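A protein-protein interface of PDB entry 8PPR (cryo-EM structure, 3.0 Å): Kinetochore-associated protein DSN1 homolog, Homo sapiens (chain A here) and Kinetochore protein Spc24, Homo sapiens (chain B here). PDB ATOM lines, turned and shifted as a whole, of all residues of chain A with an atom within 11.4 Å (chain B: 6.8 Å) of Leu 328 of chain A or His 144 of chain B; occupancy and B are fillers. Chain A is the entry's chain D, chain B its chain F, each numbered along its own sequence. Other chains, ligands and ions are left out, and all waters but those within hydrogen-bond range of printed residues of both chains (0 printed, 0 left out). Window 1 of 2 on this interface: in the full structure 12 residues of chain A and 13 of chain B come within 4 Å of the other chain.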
ATOM      1  N   SER A 317       8.221 -38.751 -25.278  1.00  0.00           N
ATOM      2  CA  SER A 317       7.347 -37.801 -24.601  1.00  0.00           C
ATOM      3  C   SER A 317       7.602 -37.784 -23.100  1.00  0.00           C
ATOM      4  O   SER A 317       7.679 -36.710 -22.493  1.00  0.00           O
ATOM      5  CB  SER A 317       5.887 -38.137 -24.893  1.00  0.00           C
ATOM      6  OG  SER A 317       5.015 -37.238 -24.234  1.00  0.00           O
ATOM      7  N   VAL A 318       7.735 -38.959 -22.483  1.00  0.00           N
ATOM      8  CA  VAL A 318       7.990 -38.983 -21.047  1.00  0.00           C
ATOM      9  C   VAL A 318       9.389 -38.464 -20.740  1.00  0.00           C
ATOM     10  O   VAL A 318       9.603 -37.826 -19.701  1.00  0.00           O
ATOM     11  CB  VAL A 318       7.752 -40.390 -20.462  1.00  0.00           C
ATOM     12  CG1 VAL A 318       6.345 -40.863 -20.788  1.00  0.00           C
ATOM     13  CG2 VAL A 318       8.781 -41.383 -20.966  1.00  0.00           C
ATOM     14  N   LEU A 320      10.899 -36.037 -22.427  1.00  0.00           N
ATOM     15  CA  LEU A 320      10.754 -34.589 -22.503  1.00  0.00           C
ATOM     16  C   LEU A 320      10.033 -34.048 -21.279  1.00  0.00           C
ATOM     17  O   LEU A 320      10.398 -32.992 -20.745  1.00  0.00           O
ATOM     18  CB  LEU A 320      10.008 -34.208 -23.779  1.00  0.00           C
ATOM     19  CG  LEU A 320       9.879 -32.712 -24.048  1.00  0.00           C
ATOM     20  CD1 LEU A 320      11.254 -32.099 -24.243  1.00  0.00           C
ATOM     21  CD2 LEU A 320       9.001 -32.473 -25.263  1.00  0.00           C
ATOM     22  N   GLY A 321       9.002 -34.760 -20.822  1.00  0.00           N
ATOM     23  CA  GLY A 321       8.313 -34.351 -19.614  1.00  0.00           C
ATOM     24  C   GLY A 321       9.233 -34.318 -18.410  1.00  0.00           C
ATOM     25  O   GLY A 321       9.217 -33.362 -17.638  1.00  0.00           O
ATOM     26  N   LYS A 322      10.057 -35.356 -18.244  1.00  0.00           N
ATOM     27  CA  LYS A 322      11.002 -35.383 -17.131  1.00  0.00           C
ATOM     28  C   LYS A 322      12.021 -34.257 -17.242  1.00  0.00           C
ATOM     29  O   LYS A 322      12.399 -33.643 -16.234  1.00  0.00           O
ATOM     30  CB  LYS A 322      11.709 -36.736 -17.083  1.00  0.00           C
ATOM     31  CG  LYS A 322      12.604 -36.921 -15.873  1.00  0.00           C
ATOM     32  CD  LYS A 322      13.283 -38.277 -15.906  1.00  0.00           C
ATOM     33  CE  LYS A 322      12.281 -39.397 -15.685  1.00  0.00           C
ATOM     34  NZ  LYS A 322      11.701 -39.367 -14.315  1.00  0.00           N
ATOM     35  N   ARG A 323      12.497 -33.989 -18.460  1.00  0.00           N
ATOM     36  CA  ARG A 323      13.435 -32.892 -18.663  1.00  0.00           C
ATOM     37  C   ARG A 323      12.812 -31.565 -18.257  1.00  0.00           C
ATOM     38  O   ARG A 323      13.474 -30.717 -17.645  1.00  0.00           O
ATOM     39  CB  ARG A 323      13.881 -32.853 -20.124  1.00  0.00           C
ATOM     40  CG  ARG A 323      14.570 -31.564 -20.528  1.00  0.00           C
ATOM     41  CD  ARG A 323      15.286 -31.717 -21.856  1.00  0.00           C
ATOM     42  NE  ARG A 323      15.942 -30.481 -22.261  1.00  0.00           N
ATOM     43  CZ  ARG A 323      15.404 -29.584 -23.075  1.00  0.00           C
ATOM     44  NH1 ARG A 323      14.196 -29.752 -23.586  1.00  0.00           N
ATOM     45  NH2 ARG A 323      16.096 -28.491 -23.385  1.00  0.00           N
ATOM     46  N   SER A 324      11.537 -31.367 -18.590  1.00  0.00           N
ATOM     47  CA  SER A 324      10.839 -30.167 -18.142  1.00  0.00           C
ATOM     48  C   SER A 324      10.668 -30.159 -16.627  1.00  0.00           C
ATOM     49  O   SER A 324      10.811 -29.110 -15.987  1.00  0.00           O
ATOM     50  CB  SER A 324       9.484 -30.063 -18.838  1.00  0.00           C
ATOM     51  OG  SER A 324       8.825 -28.858 -18.492  1.00  0.00           O
ATOM     52  N   MET A 325      10.373 -31.318 -16.035  1.00  0.00           N
ATOM     53  CA  MET A 325      10.077 -31.411 -14.610  1.00  0.00           C
ATOM     54  C   MET A 325      11.298 -31.194 -13.733  1.00  0.00           C
ATOM     55  O   MET A 325      11.141 -30.794 -12.574  1.00  0.00           O
ATOM     56  CB  MET A 325       9.505 -32.788 -14.256  1.00  0.00           C
ATOM     57  CG  MET A 325       8.156 -33.147 -14.852  1.00  0.00           C
ATOM     58  SD  MET A 325       6.786 -32.083 -14.383  1.00  0.00           S
ATOM     59  CE  MET A 325       6.643 -31.093 -15.866  1.00  0.00           C
ATOM     60  N   GLN A 326      12.497 -31.465 -14.250  1.00  0.00           N
ATOM     61  CA  GLN A 326      13.685 -31.489 -13.405  1.00  0.00           C
ATOM     62  C   GLN A 326      13.962 -30.159 -12.712  1.00  0.00           C
ATOM     63  O   GLN A 326      14.628 -30.146 -11.673  1.00  0.00           O
ATOM     64  CB  GLN A 326      14.898 -31.904 -14.234  1.00  0.00           C
ATOM     65  CG  GLN A 326      15.483 -30.787 -15.073  1.00  0.00           C
ATOM     66  CD  GLN A 326      16.883 -31.100 -15.545  1.00  0.00           C
ATOM     67  OE1 GLN A 326      17.379 -32.209 -15.354  1.00  0.00           O
ATOM     68  NE2 GLN A 326      17.531 -30.121 -16.163  1.00  0.00           N
ATOM     69  N   GLN A 327      13.472 -29.044 -13.258  1.00  0.00           N
ATOM     70  CA  GLN A 327      13.727 -27.748 -12.638  1.00  0.00           C
ATOM     71  C   GLN A 327      12.856 -27.513 -11.411  1.00  0.00           C
ATOM     72  O   GLN A 327      13.282 -26.824 -10.478  1.00  0.00           O
ATOM     73  CB  GLN A 327      13.503 -26.627 -13.652  1.00  0.00           C
ATOM     74  CG  GLN A 327      14.408 -26.704 -14.865  1.00  0.00           C
ATOM     75  CD  GLN A 327      13.733 -26.200 -16.122  1.00  0.00           C
ATOM     76  OE1 GLN A 327      12.506 -26.162 -16.210  1.00  0.00           O
ATOM     77  NE2 GLN A 327      14.535 -25.815 -17.109  1.00  0.00           N
ATOM     78  N   LEU A 328      11.650 -28.069 -11.395  1.00  0.00           N
ATOM     79  CA  LEU A 328      10.693 -27.779 -10.338  1.00  0.00           C
ATOM     80  C   LEU A 328      11.087 -28.468  -9.035  1.00  0.00           C
ATOM     81  O   LEU A 328      11.869 -29.423  -9.011  1.00  0.00           O
ATOM     82  CB  LEU A 328       9.289 -28.224 -10.748  1.00  0.00           C
ATOM     83  CG  LEU A 328       8.560 -27.409 -11.817  1.00  0.00           C
ATOM     84  CD1 LEU A 328       9.006 -27.827 -13.210  1.00  0.00           C
ATOM     85  CD2 LEU A 328       7.054 -27.556 -11.669  1.00  0.00           C
ATOM     86  N   ASP A 329      10.529 -27.963  -7.937  1.00  0.00           N
ATOM     87  CA  ASP A 329      10.658 -28.628  -6.655  1.00  0.00           C
ATOM     88  C   ASP A 329       9.765 -29.869  -6.613  1.00  0.00           C
ATOM     89  O   ASP A 329       8.831 -29.999  -7.407  1.00  0.00           O
ATOM     90  CB  ASP A 329      10.320 -27.660  -5.517  1.00  0.00           C
ATOM     91  CG  ASP A 329       8.886 -27.150  -5.569  1.00  0.00           C
ATOM     92  OD1 ASP A 329       8.122 -27.553  -6.468  1.00  0.00           O
ATOM     93  OD2 ASP A 329       8.520 -26.339  -4.694  1.00  0.00           O
ATOM     94  N   PRO A 330      10.058 -30.816  -5.715  1.00  0.00           N
ATOM     95  CA  PRO A 330       9.220 -32.026  -5.647  1.00  0.00           C
ATOM     96  C   PRO A 330       7.754 -31.742  -5.365  1.00  0.00           C
ATOM     97  O   PRO A 330       6.882 -32.432  -5.907  1.00  0.00           O
ATOM     98  CB  PRO A 330       9.870 -32.834  -4.516  1.00  0.00           C
ATOM     99  CG  PRO A 330      11.284 -32.372  -4.495  1.00  0.00           C
ATOM    100  CD  PRO A 330      11.237 -30.913  -4.838  1.00  0.00           C
ATOM    101  N   SER A 331       7.454 -30.747  -4.535  1.00  0.00           N
ATOM    102  CA  SER A 331       6.073 -30.440  -4.165  1.00  0.00           C
ATOM    103  C   SER A 331       5.945 -28.944  -3.927  1.00  0.00           C
ATOM    104  O   SER A 331       6.333 -28.436  -2.863  1.00  0.00           O
ATOM    105  CB  SER A 331       5.635 -31.224  -2.930  1.00  0.00           C
ATOM    106  OG  SER A 331       4.275 -30.974  -2.624  1.00  0.00           O
ATOM    107  N   PRO A 332       5.410 -28.198  -4.897  1.00  0.00           N
ATOM    108  CA  PRO A 332       5.120 -26.777  -4.647  1.00  0.00           C
ATOM    109  C   PRO A 332       4.087 -26.563  -3.559  1.00  0.00           C
ATOM    110  O   PRO A 332       4.062 -25.485  -2.954  1.00  0.00           O
ATOM    111  CB  PRO A 332       4.606 -26.276  -6.005  1.00  0.00           C
ATOM    112  CG  PRO A 332       5.057 -27.299  -7.000  1.00  0.00           C
ATOM    113  CD  PRO A 332       5.045 -28.601  -6.263  1.00  0.00           C
ATOM    114  N   ALA A 333       3.232 -27.555  -3.295  1.00  0.00           N
ATOM    115  CA  ALA A 333       2.153 -27.374  -2.331  1.00  0.00           C
ATOM    116  C   ALA A 333       2.688 -27.170  -0.919  1.00  0.00           C
ATOM    117  O   ALA A 333       2.229 -26.277  -0.200  1.00  0.00           O
ATOM    118  CB  ALA A 333       1.205 -28.572  -2.375  1.00  0.00           C
ATOM    119  N   ARG A 334       3.653 -27.993  -0.500  1.00  0.00           N
ATOM    120  CA  ARG A 334       4.210 -27.855   0.841  1.00  0.00           C
ATOM    121  C   ARG A 334       4.901 -26.510   1.007  1.00  0.00           C
ATOM    122  O   ARG A 334       4.725 -25.824   2.021  1.00  0.00           O
ATOM    123  CB  ARG A 334       5.191 -28.991   1.122  1.00  0.00           C
ATOM    124  CG  ARG A 334       4.733 -30.340   0.621  1.00  0.00           C
ATOM    125  CD  ARG A 334       5.585 -31.455   1.193  1.00  0.00           C
ATOM    126  NE  ARG A 334       5.108 -31.879   2.503  1.00  0.00           N
ATOM    127  CZ  ARG A 334       4.137 -32.761   2.696  1.00  0.00           C
ATOM    128  NH1 ARG A 334       3.516 -33.338   1.682  1.00  0.00           N
ATOM    129  NH2 ARG A 334       3.783 -33.072   3.938  1.00  0.00           N
ATOM    130  N   LYS A 335       5.697 -26.121   0.012  1.00  0.00           N
ATOM    131  CA  LYS A 335       6.417 -24.856   0.083  1.00  0.00           C
ATOM    132  C   LYS A 335       5.453 -23.678   0.119  1.00  0.00           C
ATOM    133  O   LYS A 335       5.674 -22.705   0.846  1.00  0.00           O
ATOM    134  CB  LYS A 335       7.365 -24.739  -1.108  1.00  0.00           C
ATOM    135  CG  LYS A 335       8.403 -25.842  -1.181  1.00  0.00           C
ATOM    136  CD  LYS A 335       9.653 -25.483  -0.404  1.00  0.00           C
ATOM    137  CE  LYS A 335      10.767 -26.474  -0.686  1.00  0.00           C
ATOM    138  NZ  LYS A 335      10.299 -27.882  -0.544  1.00  0.00           N
ATOM    139  N   LEU A 336       4.382 -23.746  -0.672  1.00  0.00           N
ATOM    140  CA  LEU A 336       3.398 -22.671  -0.681  1.00  0.00           C
ATOM    141  C   LEU A 336       2.635 -22.604   0.636  1.00  0.00           C
ATOM    142  O   LEU A 336       2.369 -21.513   1.151  1.00  0.00           O
ATOM    143  CB  LEU A 336       2.440 -22.862  -1.853  1.00  0.00           C
ATOM    144  CG  LEU A 336       1.470 -21.718  -2.142  1.00  0.00           C
ATOM    145  CD1 LEU A 336       2.234 -20.427  -2.381  1.00  0.00           C
ATOM    146  CD2 LEU A 336       0.611 -22.065  -3.342  1.00  0.00           C
ATOM    147  N   TYR B 138       6.014 -20.388  -6.549  1.00  0.00           N
ATOM    148  CA  TYR B 138       5.401 -21.648  -6.158  1.00  0.00           C
ATOM    149  C   TYR B 138       3.960 -21.766  -6.624  1.00  0.00           C
ATOM    150  O   TYR B 138       3.524 -22.869  -6.966  1.00  0.00           O
ATOM    151  CB  TYR B 138       5.481 -21.828  -4.641  1.00  0.00           C
ATOM    152  CG  TYR B 138       6.889 -22.101  -4.162  1.00  0.00           C
ATOM    153  CD1 TYR B 138       7.799 -22.763  -4.977  1.00  0.00           C
ATOM    154  CD2 TYR B 138       7.316 -21.683  -2.910  1.00  0.00           C
ATOM    155  CE1 TYR B 138       9.089 -23.012  -4.552  1.00  0.00           C
ATOM    156  CE2 TYR B 138       8.607 -21.922  -2.479  1.00  0.00           C
ATOM    157  CZ  TYR B 138       9.487 -22.591  -3.303  1.00  0.00           C
ATOM    158  OH  TYR B 138      10.772 -22.836  -2.877  1.00  0.00           O
ATOM    159  N   VAL B 139       3.214 -20.661  -6.674  1.00  0.00           N
ATOM    160  CA  VAL B 139       1.866 -20.698  -7.233  1.00  0.00           C
ATOM    161  C   VAL B 139       1.915 -21.076  -8.706  1.00  0.00           C
ATOM    162  O   VAL B 139       1.137 -21.915  -9.174  1.00  0.00           O
ATOM    163  CB  VAL B 139       1.159 -19.348  -7.022  1.00  0.00           C
ATOM    164  CG1 VAL B 139      -0.002 -19.197  -7.990  1.00  0.00           C
ATOM    165  CG2 VAL B 139       0.666 -19.229  -5.593  1.00  0.00           C
ATOM    166  N   ALA B 140       2.829 -20.462  -9.460  1.00  0.00           N
ATOM    167  CA  ALA B 140       2.949 -20.788 -10.876  1.00  0.00           C
ATOM    168  C   ALA B 140       3.376 -22.236 -11.075  1.00  0.00           C
ATOM    169  O   ALA B 140       2.843 -22.933 -11.947  1.00  0.00           O
ATOM    170  CB  ALA B 140       3.935 -19.836 -11.549  1.00  0.00           C
ATOM    171  N   GLN B 141       4.331 -22.708 -10.272  1.00  0.00           N
ATOM    172  CA  GLN B 141       4.784 -24.088 -10.403  1.00  0.00           C
ATOM    173  C   GLN B 141       3.683 -25.070 -10.028  1.00  0.00           C
ATOM    174  O   GLN B 141       3.555 -26.128 -10.650  1.00  0.00           O
ATOM    175  CB  GLN B 141       6.034 -24.316  -9.557  1.00  0.00           C
ATOM    176  CG  GLN B 141       7.255 -23.568 -10.068  1.00  0.00           C
ATOM    177  CD  GLN B 141       8.550 -24.077  -9.469  1.00  0.00           C
ATOM    178  OE1 GLN B 141       8.542 -24.885  -8.540  1.00  0.00           O
ATOM    179  NE2 GLN B 141       9.673 -23.609 -10.002  1.00  0.00           N
ATOM    180  N   LEU B 142       2.878 -24.740  -9.017  1.00  0.00           N
ATOM    181  CA  LEU B 142       1.754 -25.595  -8.660  1.00  0.00           C
ATOM    182  C   LEU B 142       0.700 -25.605  -9.761  1.00  0.00           C
ATOM    183  O   LEU B 142       0.144 -26.662 -10.084  1.00  0.00           O
ATOM    184  CB  LEU B 142       1.156 -25.133  -7.333  1.00  0.00           C
ATOM    185  CG  LEU B 142      -0.162 -25.781  -6.914  1.00  0.00           C
ATOM    186  CD1 LEU B 142       0.085 -27.194  -6.415  1.00  0.00           C
ATOM    187  CD2 LEU B 142      -0.848 -24.944  -5.849  1.00  0.00           C
ATOM    188  N   TYR B 143       0.419 -24.439 -10.351  1.00  0.00           N
ATOM    189  CA  TYR B 143      -0.463 -24.375 -11.512  1.00  0.00           C
ATOM    190  C   TYR B 143       0.029 -25.299 -12.615  1.00  0.00           C
ATOM    191  O   TYR B 143      -0.740 -26.085 -13.181  1.00  0.00           O
ATOM    192  CB  TYR B 143      -0.538 -22.941 -12.038  1.00  0.00           C
ATOM    193  CG  TYR B 143      -1.690 -22.109 -11.524  1.00  0.00           C
ATOM    194  CD1 TYR B 143      -3.004 -22.513 -11.711  1.00  0.00           C
ATOM    195  CD2 TYR B 143      -1.461 -20.900 -10.880  1.00  0.00           C
ATOM    196  CE1 TYR B 143      -4.059 -21.745 -11.253  1.00  0.00           C
ATOM    197  CE2 TYR B 143      -2.509 -20.126 -10.419  1.00  0.00           C
ATOM    198  CZ  TYR B 143      -3.806 -20.554 -10.607  1.00  0.00           C
ATOM    199  OH  TYR B 143      -4.854 -19.788 -10.150  1.00  0.00           O
ATOM    200  N   HIS B 144       1.319 -25.212 -12.932  1.00  0.00           N
ATOM    201  CA  HIS B 144       1.867 -25.997 -14.032  1.00  0.00           C
ATOM    202  C   HIS B 144       1.852 -27.485 -13.710  1.00  0.00           C
ATOM    203  O   HIS B 144       1.543 -28.310 -14.575  1.00  0.00           O
ATOM    204  CB  HIS B 144       3.282 -25.525 -14.352  1.00  0.00           C
ATOM    205  CG  HIS B 144       4.027 -26.436 -15.272  1.00  0.00           C
ATOM    206  ND1 HIS B 144       4.856 -27.438 -14.818  1.00  0.00           N
ATOM    207  CD2 HIS B 144       4.057 -26.505 -16.624  1.00  0.00           C
ATOM    208  CE1 HIS B 144       5.372 -28.076 -15.852  1.00  0.00           C
ATOM    209  NE2 HIS B 144       4.901 -27.533 -16.959  1.00  0.00           N
ATOM    210  N   GLN B 145       2.184 -27.846 -12.469  1.00  0.00           N
ATOM    211  CA  GLN B 145       2.130 -29.243 -12.058  1.00  0.00           C
ATOM    212  C   GLN B 145       0.717 -29.792 -12.150  1.00  0.00           C
ATOM    213  O   GLN B 145       0.518 -30.932 -12.586  1.00  0.00           O
ATOM    214  CB  GLN B 145       2.659 -29.385 -10.630  1.00  0.00           C
ATOM    215  CG  GLN B 145       2.345 -30.720  -9.982  1.00  0.00           C
ATOM    216  CD  GLN B 145       3.207 -30.994  -8.767  1.00  0.00           C
ATOM    217  OE1 GLN B 145       2.719 -31.007  -7.637  1.00  0.00           O
ATOM    218  NE2 GLN B 145       4.496 -31.212  -8.993  1.00  0.00           N
ATOM    219  N   VAL B 146      -0.273 -28.996 -11.754  1.00  0.00           N
ATOM    220  CA  VAL B 146      -1.660 -29.429 -11.850  1.00  0.00           C
ATOM    221  C   VAL B 146      -2.071 -29.582 -13.307  1.00  0.00           C
ATOM    222  O   VAL B 146      -2.781 -30.527 -13.672  1.00  0.00           O
ATOM    223  CB  VAL B 146      -2.566 -28.436 -11.103  1.00  0.00           C
ATOM    224  CG1 VAL B 146      -4.004 -28.572 -11.566  1.00  0.00           C
ATOM    225  CG2 VAL B 146      -2.447 -28.648  -9.604  1.00  0.00           C
ATOM    226  N   SER B 147      -1.622 -28.669 -14.166  1.00  0.00           N
ATOM    227  CA  SER B 147      -2.058 -28.653 -15.554  1.00  0.00           C
ATOM    228  C   SER B 147      -1.127 -29.398 -16.497  1.00  0.00           C
ATOM    229  O   SER B 147      -1.592 -29.883 -17.535  1.00  0.00           O
ATOM    230  CB  SER B 147      -2.199 -27.208 -16.041  1.00  0.00           C
ATOM    231  OG  SER B 147      -1.027 -26.467 -15.757  1.00  0.00           O
ATOM    232  N   LYS B 148       0.161 -29.511 -16.164  1.00  0.00           N
ATOM    233  CA  LYS B 148       1.161 -30.080 -17.070  1.00  0.00           C
ATOM    234  C   LYS B 148       1.155 -29.347 -18.409  1.00  0.00           C
ATOM    235  O   LYS B 148       1.324 -29.946 -19.472  1.00  0.00           O
ATOM    236  CB  LYS B 148       0.949 -31.582 -17.266  1.00  0.00           C
ATOM    237  CG  LYS B 148       1.000 -32.381 -15.978  1.00  0.00           C
ATOM    238  CD  LYS B 148       0.776 -33.858 -16.243  1.00  0.00           C
ATOM    239  CE  LYS B 148       2.027 -34.505 -16.809  1.00  0.00           C
ATOM    240  NZ  LYS B 148       3.132 -34.535 -15.812  1.00  0.00           N
ATOM    241  N   ILE B 149       0.954 -28.033 -18.348  1.00  0.00           N
ATOM    242  CA  ILE B 149       0.830 -27.187 -19.525  1.00  0.00           C
ATOM    243  C   ILE B 149       1.877 -26.088 -19.456  1.00  0.00           C
ATOM    244  O   ILE B 149       1.991 -25.388 -18.445  1.00  0.00           O
ATOM    245  CB  ILE B 149      -0.582 -26.580 -19.634  1.00  0.00           C
ATOM    246  CG1 ILE B 149      -1.625 -27.686 -19.812  1.00  0.00           C
ATOM    247  CG2 ILE B 149      -0.637 -25.550 -20.750  1.00  0.00           C
ATOM    248  CD1 ILE B 149      -3.026 -27.175 -20.047  1.00  0.00           C
ATOM    249  N   GLU B 150       2.630 -25.930 -20.540  1.00  0.00           N
ATOM    250  CA  GLU B 150       3.638 -24.886 -20.657  1.00  0.00           C
ATOM    251  C   GLU B 150       3.179 -23.907 -21.725  1.00  0.00           C
ATOM    252  O   GLU B 150       2.939 -24.306 -22.869  1.00  0.00           O
ATOM    253  CB  GLU B 150       5.001 -25.478 -21.016  1.00  0.00           C
ATOM    254  CG  GLU B 150       5.433 -26.610 -20.105  1.00  0.00           C
ATOM    255  CD  GLU B 150       6.794 -27.161 -20.470  1.00  0.00           C
ATOM    256  OE1 GLU B 150       7.541 -26.472 -21.196  1.00  0.00           O
ATOM    257  OE2 GLU B 150       7.115 -28.286 -20.036  1.00  0.00           O
ATOM    258  N   TRP B 151       3.060 -22.639 -21.356  1.00  0.00           N
ATOM    259  CA  TRP B 151       2.540 -21.631 -22.265  1.00  0.00           C
ATOM    260  C   TRP B 151       3.646 -21.043 -23.132  1.00  0.00           C
ATOM    261  O   TRP B 151       4.825 -21.047 -22.776  1.00  0.00           O
ATOM    262  CB  TRP B 151       1.846 -20.510 -21.493  1.00  0.00           C
ATOM    263  CG  TRP B 151       0.790 -20.996 -20.568  1.00  0.00           C
ATOM    264  CD1 TRP B 151       0.824 -20.988 -19.206  1.00  0.00           C
ATOM    265  CD2 TRP B 151      -0.467 -21.566 -20.936  1.00  0.00           C
ATOM    266  NE1 TRP B 151      -0.338 -21.517 -18.701  1.00  0.00           N
ATOM    267  CE2 TRP B 151      -1.147 -21.881 -19.745  1.00  0.00           C
ATOM    268  CE3 TRP B 151      -1.085 -21.840 -22.159  1.00  0.00           C
ATOM    269  CZ2 TRP B 151      -2.414 -22.457 -19.740  1.00  0.00           C
ATOM    270  CZ3 TRP B 151      -2.340 -22.411 -22.153  1.00  0.00           C
ATOM    271  CH2 TRP B 151      -2.991 -22.715 -20.952  1.00  0.00           C
ATOM    272  N   ILE B 163       2.243 -26.330 -24.859  1.00  0.00           N
ATOM    273  CA  ILE B 163       2.483 -27.766 -24.917  1.00  0.00           C
ATOM    274  C   ILE B 163       1.725 -28.429 -23.779  1.00  0.00           C
ATOM    275  O   ILE B 163       1.833 -28.003 -22.623  1.00  0.00           O
ATOM    276  CB  ILE B 163       3.985 -28.092 -24.827  1.00  0.00           C
ATOM    277  CG1 ILE B 163       4.729 -27.515 -26.033  1.00  0.00           C
ATOM    278  CG2 ILE B 163       4.197 -29.591 -24.696  1.00  0.00           C
ATOM    279  CD1 ILE B 163       6.234 -27.524 -25.882  1.00  0.00           C
ATOM    280  N   HIS B 165       1.351 -31.803 -21.640  1.00  0.00           N
ATOM    281  CA  HIS B 165       1.994 -33.047 -21.252  1.00  0.00           C
ATOM    282  C   HIS B 165       1.019 -34.033 -20.625  1.00  0.00           C
ATOM    283  O   HIS B 165       1.437 -35.108 -20.181  1.00  0.00           O
ATOM    284  CB  HIS B 165       3.147 -32.761 -20.290  1.00  0.00           C
ATOM    285  CG  HIS B 165       4.268 -31.988 -20.909  1.00  0.00           C
ATOM    286  ND1 HIS B 165       5.390 -32.593 -21.433  1.00  0.00           N
ATOM    287  CD2 HIS B 165       4.437 -30.657 -21.095  1.00  0.00           C
ATOM    288  CE1 HIS B 165       6.204 -31.669 -21.910  1.00  0.00           C
ATOM    289  NE2 HIS B 165       5.649 -30.486 -21.718  1.00  0.00           N
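The side-chain carboxylate (OE2) of Glu 150 of chain B lies within hydrogen-bond range of a ring nitrogen (NE2) of His 165 of chain B (3.1 Å). The side-chain hydroxyl (OG) of Ser 147 of chain B sits at hydrogen-bond distance from the backbone carbonyl oxygen (O) of His 144 of chain B (3.4 Å). The backbone carbonyl oxygen (O) of Glu 150 of chain B sits at hydrogen-bond distance from the backbone NH (N) of Ile 163 of chain B (2.9 Å). OE1 of Gln 327 of chain A lies close to O of Ser 324 of chain A (3.4 Å). The backbone carbonyl oxygen (O) of Lys 148 of chain B is in hydrogen-bond range of the backbone NH (N) of His 165 of chain B (2.9 Å).
The side-chain carboxylate of Asp 329 of chain A lies close to the side-chain amide oxygen of Gln 141 of chain B (3.4 Å). The side-chain carboxylate (OE2) of Glu 150 of chain B lies close to the side-chain hydroxyl (OG) of Ser 324 of chain A (2.4 Å).
Leu 328 of chain A touches just these residues of chain B: Gln 141 (3.9 Å) and His 144 (3.8 Å). Of chain A, only Met 325 (3.3 Å) and Leu 328 (3.8 Å) come within 4 Å of His 144 of chain B. No residue of chain A comes within 4 Å of Ala 140 of chain B. No residue of chain A comes within 4 Å of Val 146 of chain B. No residue of chain A comes within 4 Å of Ser 147 of chain B. No residue of chain A comes within 4 Å of Lys 148 of chain B. Of the printed residues of chain A, Glu 150 of chain B touches Ser 324. Printed residues of chain B within 4 Å of Leu 336 of chain A: Val 139. Printed residues of chain A within 4 Å of Val 139 of chain B: Leu 336 (3.6 Å). Printed residues of chain B within 4 Å of Pro 332 of chain A: Tyr 138 (3.7 Å), Leu 142 (3.8 Å) and Gln 145 (3.6 Å). Of the printed residues of chain B, Lys 335 of chain A touches Tyr 138. Of the printed residues of chain B, Gly 321 of chain A touches His 165. The nearest residue of chain A that does not touch His 144 of chain B is Ser 324 of chain A (4.4 Å). The nearest printed residue of chain B that does not touch Lys 335 of chain A is Gln 141 of chain B (7.4 Å).
Of the 19 printed residues of chain A, 8 touch a printed residue of chain B. Hydrophobic or aromatic side chains of chain A within 4 Å of the printed part of chain B: Met 325, Leu 328, Pro 332 and Leu 336. Printed residues of chain B that touch a printed residue of chain A: Tyr 138, Val 139, Gln 141, Leu 142, His 144, Gln 145, Glu 150 and His 165. Among the printed residues, 12 pairs touch across the chains. Among the printed residues, no Asp or Glu carboxylate lies within 4 Å of a Lys or Arg side-chain nitrogen of the other chain.
Among the printed residues, merely in contact across the chains: Met 325 of chain A with His 144 of chain B (3.3 Å), Lys 335 of chain A with Tyr 138 of chain B (3.4 Å), Asp 329 of chain A with Tyr 138 of chain B (3.4 Å), Pro 332 of chain A with Gln 145 of chain B (3.6 Å), Leu 336 of chain A with Val 139 of chain B (3.6 Å), Pro 332 of chain A with Tyr 138 of chain B (3.7 Å), Pro 332 of chain A with Leu 142 of chain B (3.8 Å), Leu 328 of chain A with His 144 of chain B (3.8 Å), Gly 321 of chain A with His 165 of chain B (3.9 Å) and Leu 328 of chain A with Gln 141 of chain B (3.9 Å).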
